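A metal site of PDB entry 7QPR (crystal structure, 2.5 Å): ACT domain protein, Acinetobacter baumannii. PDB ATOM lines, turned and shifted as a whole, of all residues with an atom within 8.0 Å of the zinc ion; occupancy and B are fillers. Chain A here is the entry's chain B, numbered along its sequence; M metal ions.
The backbone NH of Arg 586 sits close to the side-chain sulfur of Cys 565, 3.2 Å away.
O of His 585 is in hydrogen-bond range of N of Gln 574 (2.9 Å).
SG of Cys 589 lies close to N of Asn 591, 3.5 Å away.
The backbone NH (N) of Ala 562 is in hydrogen-bond range of the backbone carbonyl oxygen (O) of Val 584, at 2.9 Å.
Ala 562 touches the zinc ion (CB to ZN, 3.9 Å).
Within 4 Å of the zinc ion: Ala 562, Cys 564, Cys 565, His 585 and Cys 589.
The nearest printed residue that does not touch the zinc ion is Asn 591 (4.3 Å).
The zinc ion is bound by ND1 of His 585 (2.2 Å), SG of Cys 589 (2.2 Å), SG of Cys 564 (2.3 Å) and SG of Cys 565 (2.5 Å).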
ATOM      1  N   TYR A 561      -6.528  32.129  25.994  1.00  0.00           N
ATOM      2  CA  TYR A 561      -7.050  31.329  27.102  1.00  0.00           C
ATOM      3  C   TYR A 561      -8.565  31.335  27.037  1.00  0.00           C
ATOM      4  O   TYR A 561      -9.145  32.406  26.854  1.00  0.00           O
ATOM      5  CB  TYR A 561      -6.573  31.919  28.433  1.00  0.00           C
ATOM      6  CG  TYR A 561      -5.065  31.945  28.592  1.00  0.00           C
ATOM      7  CD1 TYR A 561      -4.307  30.816  28.368  1.00  0.00           C
ATOM      8  CD2 TYR A 561      -4.416  33.085  29.036  1.00  0.00           C
ATOM      9  CE1 TYR A 561      -2.928  30.827  28.532  1.00  0.00           C
ATOM     10  CE2 TYR A 561      -3.038  33.115  29.187  1.00  0.00           C
ATOM     11  CZ  TYR A 561      -2.302  31.980  28.928  1.00  0.00           C
ATOM     12  OH  TYR A 561      -0.942  31.996  29.098  1.00  0.00           O
ATOM     13  N   ALA A 562      -9.218  30.180  27.188  1.00  0.00           N
ATOM     14  CA  ALA A 562     -10.684  30.082  27.102  1.00  0.00           C
ATOM     15  C   ALA A 562     -11.366  30.747  28.272  1.00  0.00           C
ATOM     16  O   ALA A 562     -10.995  30.494  29.409  1.00  0.00           O
ATOM     17  CB  ALA A 562     -11.112  28.635  27.031  1.00  0.00           C
ATOM     18  N   HIS A 563     -12.382  31.575  28.006  1.00  0.00           N
ATOM     19  CA  HIS A 563     -13.111  32.294  29.065  1.00  0.00           C
ATOM     20  C   HIS A 563     -14.103  31.429  29.846  1.00  0.00           C
ATOM     21  O   HIS A 563     -14.609  31.875  30.862  1.00  0.00           O
ATOM     22  CB  HIS A 563     -13.798  33.536  28.514  1.00  0.00           C
ATOM     23  CG  HIS A 563     -12.864  34.568  27.950  1.00  0.00           C
ATOM     24  ND1 HIS A 563     -13.327  35.653  27.228  1.00  0.00           N
ATOM     25  CD2 HIS A 563     -11.510  34.656  28.024  1.00  0.00           C
ATOM     26  CE1 HIS A 563     -12.259  36.355  26.879  1.00  0.00           C
ATOM     27  NE2 HIS A 563     -11.143  35.782  27.335  1.00  0.00           N
ATOM     28  N   CYS A 564     -14.373  30.205  29.368  1.00  0.00           N
ATOM     29  CA  CYS A 564     -15.298  29.279  29.996  1.00  0.00           C
ATOM     30  C   CYS A 564     -14.683  28.626  31.234  1.00  0.00           C
ATOM     31  O   CYS A 564     -15.375  28.368  32.223  1.00  0.00           O
ATOM     32  CB  CYS A 564     -15.789  28.227  28.997  1.00  0.00           C
ATOM     33  SG  CYS A 564     -14.483  27.516  27.968  1.00  0.00           S
ATOM     34  N   CYS A 565     -13.375  28.319  31.167  1.00  0.00           N
ATOM     35  CA  CYS A 565     -12.660  27.604  32.219  1.00  0.00           C
ATOM     36  C   CYS A 565     -11.481  28.371  32.808  1.00  0.00           C
ATOM     37  O   CYS A 565     -11.058  28.068  33.936  1.00  0.00           O
ATOM     38  CB  CYS A 565     -12.209  26.235  31.715  1.00  0.00           C
ATOM     39  SG  CYS A 565     -11.384  26.281  30.103  1.00  0.00           S
ATOM     40  N   ASN A 566     -10.940  29.347  32.050  1.00  0.00           N
ATOM     41  CA  ASN A 566      -9.798  30.189  32.445  1.00  0.00           C
ATOM     42  C   ASN A 566      -8.639  29.377  33.013  1.00  0.00           C
ATOM     43  O   ASN A 566      -8.410  29.374  34.222  1.00  0.00           O
ATOM     44  CB  ASN A 566     -10.218  31.292  33.404  1.00  0.00           C
ATOM     45  CG  ASN A 566     -11.189  32.268  32.795  1.00  0.00           C
ATOM     46  OD1 ASN A 566     -12.399  32.119  32.906  1.00  0.00           O
ATOM     47  ND2 ASN A 566     -10.667  33.285  32.122  1.00  0.00           N
ATOM     48  N   PRO A 567      -7.902  28.658  32.145  1.00  0.00           N
ATOM     49  CA  PRO A 567      -6.769  27.860  32.622  1.00  0.00           C
ATOM     50  C   PRO A 567      -5.624  28.691  33.201  1.00  0.00           C
ATOM     51  O   PRO A 567      -5.319  29.758  32.683  1.00  0.00           O
ATOM     52  CB  PRO A 567      -6.338  27.066  31.380  1.00  0.00           C
ATOM     53  CG  PRO A 567      -6.791  27.914  30.234  1.00  0.00           C
ATOM     54  CD  PRO A 567      -8.062  28.557  30.681  1.00  0.00           C
ATOM     55  N   GLN A 574      -5.687  21.366  27.532  1.00  0.00           N
ATOM     56  CA  GLN A 574      -5.852  20.851  26.196  1.00  0.00           C
ATOM     57  C   GLN A 574      -6.294  21.993  25.274  1.00  0.00           C
ATOM     58  O   GLN A 574      -7.145  22.784  25.644  1.00  0.00           O
ATOM     59  CB  GLN A 574      -6.856  19.702  26.181  1.00  0.00           C
ATOM     60  CG  GLN A 574      -6.758  18.836  24.941  1.00  0.00           C
ATOM     61  CD  GLN A 574      -6.899  17.370  25.276  1.00  0.00           C
ATOM     62  OE1 GLN A 574      -7.856  16.924  25.918  1.00  0.00           O
ATOM     63  NE2 GLN A 574      -5.924  16.593  24.850  1.00  0.00           N
ATOM     64  N   ILE A 583      -7.182  27.831  21.174  1.00  0.00           N
ATOM     65  CA  ILE A 583      -7.881  28.191  22.402  1.00  0.00           C
ATOM     66  C   ILE A 583      -7.543  27.179  23.489  1.00  0.00           C
ATOM     67  O   ILE A 583      -7.892  26.010  23.363  1.00  0.00           O
ATOM     68  CB  ILE A 583      -9.403  28.290  22.194  1.00  0.00           C
ATOM     69  CG1 ILE A 583      -9.766  29.105  20.946  1.00  0.00           C
ATOM     70  CG2 ILE A 583     -10.078  28.824  23.428  1.00  0.00           C
ATOM     71  CD1 ILE A 583      -9.204  30.494  20.872  1.00  0.00           C
ATOM     72  N   VAL A 584      -6.813  27.600  24.512  1.00  0.00           N
ATOM     73  CA  VAL A 584      -6.399  26.721  25.592  1.00  0.00           C
ATOM     74  C   VAL A 584      -7.479  26.573  26.635  1.00  0.00           C
ATOM     75  O   VAL A 584      -7.971  27.556  27.145  1.00  0.00           O
ATOM     76  CB  VAL A 584      -5.056  27.178  26.176  1.00  0.00           C
ATOM     77  CG1 VAL A 584      -4.620  26.267  27.307  1.00  0.00           C
ATOM     78  CG2 VAL A 584      -4.010  27.218  25.088  1.00  0.00           C
ATOM     79  N   HIS A 585      -7.896  25.323  26.912  1.00  0.00           N
ATOM     80  CA  HIS A 585      -8.943  24.997  27.867  1.00  0.00           C
ATOM     81  C   HIS A 585      -8.401  24.061  28.944  1.00  0.00           C
ATOM     82  O   HIS A 585      -7.441  23.337  28.707  1.00  0.00           O
ATOM     83  CB  HIS A 585     -10.069  24.218  27.154  1.00  0.00           C
ATOM     84  CG  HIS A 585     -10.893  25.005  26.182  1.00  0.00           C
ATOM     85  ND1 HIS A 585     -12.074  25.594  26.575  1.00  0.00           N
ATOM     86  CD2 HIS A 585     -10.729  25.193  24.855  1.00  0.00           C
ATOM     87  CE1 HIS A 585     -12.560  26.170  25.487  1.00  0.00           C
ATOM     88  NE2 HIS A 585     -11.793  25.931  24.428  1.00  0.00           N
ATOM     89  N   ARG A 586      -9.054  24.033  30.116  1.00  0.00           N
ATOM     90  CA  ARG A 586      -8.705  23.084  31.166  1.00  0.00           C
ATOM     91  C   ARG A 586      -9.281  21.706  30.759  1.00  0.00           C
ATOM     92  O   ARG A 586     -10.364  21.642  30.187  1.00  0.00           O
ATOM     93  CB  ARG A 586      -9.303  23.536  32.493  1.00  0.00           C
ATOM     94  CG  ARG A 586      -8.470  24.576  33.201  1.00  0.00           C
ATOM     95  CD  ARG A 586      -9.177  25.086  34.450  1.00  0.00           C
ATOM     96  NE  ARG A 586      -9.060  24.149  35.570  1.00  0.00           N
ATOM     97  CZ  ARG A 586      -9.701  24.280  36.720  1.00  0.00           C
ATOM     98  NH1 ARG A 586     -10.528  25.310  36.922  1.00  0.00           N
ATOM     99  NH2 ARG A 586      -9.538  23.387  37.688  1.00  0.00           N
ATOM    100  N   ILE A 587      -8.541  20.618  31.050  1.00  0.00           N
ATOM    101  CA  ILE A 587      -8.863  19.215  30.718  1.00  0.00           C
ATOM    102  C   ILE A 587     -10.340  18.812  30.979  1.00  0.00           C
ATOM    103  O   ILE A 587     -10.914  18.114  30.141  1.00  0.00           O
ATOM    104  CB  ILE A 587      -7.845  18.272  31.455  1.00  0.00           C
ATOM    105  CG1 ILE A 587      -6.571  18.028  30.615  1.00  0.00           C
ATOM    106  CG2 ILE A 587      -8.434  16.950  31.968  1.00  0.00           C
ATOM    107  CD1 ILE A 587      -6.712  17.143  29.442  1.00  0.00           C
ATOM    108  N   ARG A 588     -10.948  19.239  32.088  1.00  0.00           N
ATOM    109  CA  ARG A 588     -12.325  18.849  32.418  1.00  0.00           C
ATOM    110  C   ARG A 588     -13.376  19.918  32.101  1.00  0.00           C
ATOM    111  O   ARG A 588     -14.373  20.021  32.825  1.00  0.00           O
ATOM    112  CB  ARG A 588     -12.409  18.437  33.895  1.00  0.00           C
ATOM    113  N   CYS A 589     -13.137  20.752  31.088  1.00  0.00           N
ATOM    114  CA  CYS A 589     -14.093  21.789  30.721  1.00  0.00           C
ATOM    115  C   CYS A 589     -15.228  21.167  29.920  1.00  0.00           C
ATOM    116  O   CYS A 589     -14.997  20.301  29.095  1.00  0.00           O
ATOM    117  CB  CYS A 589     -13.429  22.923  29.956  1.00  0.00           C
ATOM    118  SG  CYS A 589     -14.567  24.228  29.393  1.00  0.00           S
ATOM    119  N   HIS A 590     -16.445  21.637  30.174  1.00  0.00           N
ATOM    120  CA  HIS A 590     -17.686  21.223  29.514  1.00  0.00           C
ATOM    121  C   HIS A 590     -17.602  21.508  28.016  1.00  0.00           C
ATOM    122  O   HIS A 590     -17.960  20.638  27.218  1.00  0.00           O
ATOM    123  CB  HIS A 590     -18.928  21.933  30.144  1.00  0.00           C
ATOM    124  CG  HIS A 590     -18.614  23.053  31.118  1.00  0.00           C
ATOM    125  ND1 HIS A 590     -18.630  24.378  30.713  1.00  0.00           N
ATOM    126  CD2 HIS A 590     -18.231  22.987  32.413  1.00  0.00           C
ATOM    127  CE1 HIS A 590     -18.278  25.083  31.788  1.00  0.00           C
ATOM    128  NE2 HIS A 590     -18.028  24.290  32.836  1.00  0.00           N
ATOM    129  N   ASN A 591     -17.114  22.704  27.626  1.00  0.00           N
ATOM    130  CA  ASN A 591     -16.979  23.129  26.235  1.00  0.00           C
ATOM    131  C   ASN A 591     -15.909  22.330  25.521  1.00  0.00           C
ATOM    132  O   ASN A 591     -16.095  21.978  24.357  1.00  0.00           O
ATOM    133  CB  ASN A 591     -16.660  24.616  26.145  1.00  0.00           C
ATOM    134  CG  ASN A 591     -17.790  25.519  26.541  1.00  0.00           C
ATOM    135  OD1 ASN A 591     -18.703  25.107  27.269  1.00  0.00           O
ATOM    136  ND2 ASN A 591     -17.756  26.755  26.079  1.00  0.00           N
ATOM    137  N   LEU A 592     -14.784  22.042  26.203  1.00  0.00           N
ATOM    138  CA  LEU A 592     -13.664  21.300  25.644  1.00  0.00           C
ATOM    139  C   LEU A 592     -14.049  19.850  25.343  1.00  0.00           C
ATOM    140  O   LEU A 592     -13.710  19.333  24.280  1.00  0.00           O
ATOM    141  CB  LEU A 592     -12.432  21.329  26.567  1.00  0.00           C
ATOM    142  CG  LEU A 592     -11.236  20.514  26.090  1.00  0.00           C
ATOM    143  CD1 LEU A 592     -10.477  21.244  25.028  1.00  0.00           C
ATOM    144  CD2 LEU A 592     -10.343  20.121  27.206  1.00  0.00           C
ATOM    145  N   LEU A 593     -14.725  19.189  26.288  1.00  0.00           N
ATOM    146  CA  LEU A 593     -15.125  17.806  26.099  1.00  0.00           C
ATOM    147  C   LEU A 593     -16.218  17.644  25.020  1.00  0.00           C
ATOM    148  O   LEU A 593     -16.290  16.600  24.388  1.00  0.00           O
ATOM    149  CB  LEU A 593     -15.513  17.152  27.435  1.00  0.00           C
ATOM    150  CG  LEU A 593     -14.416  17.246  28.535  1.00  0.00           C
ATOM    151  CD1 LEU A 593     -14.895  16.737  29.868  1.00  0.00           C
ATOM    152  CD2 LEU A 593     -13.170  16.503  28.135  1.00  0.00           C
ATOM    153  N   ASP A 689     -14.618  28.115  37.545  1.00  0.00           N
ATOM    154  CA  ASP A 689     -14.034  28.003  36.207  1.00  0.00           C
ATOM    155  C   ASP A 689     -14.055  29.380  35.557  1.00  0.00           C
ATOM    156  O   ASP A 689     -13.103  29.756  34.875  1.00  0.00           O
ATOM    157  CB  ASP A 689     -14.792  26.966  35.365  1.00  0.00           C
ATOM    158  CG  ASP A 689     -14.192  25.569  35.436  1.00  0.00           C
ATOM    159  OD1 ASP A 689     -12.973  25.439  35.187  1.00  0.00           O
ATOM    160  OD2 ASP A 689     -14.946  24.608  35.622  1.00  0.00           O
HETATM  161 ZN    ZN M   1     -13.207  25.706  28.462  1.00  0.00          ZN
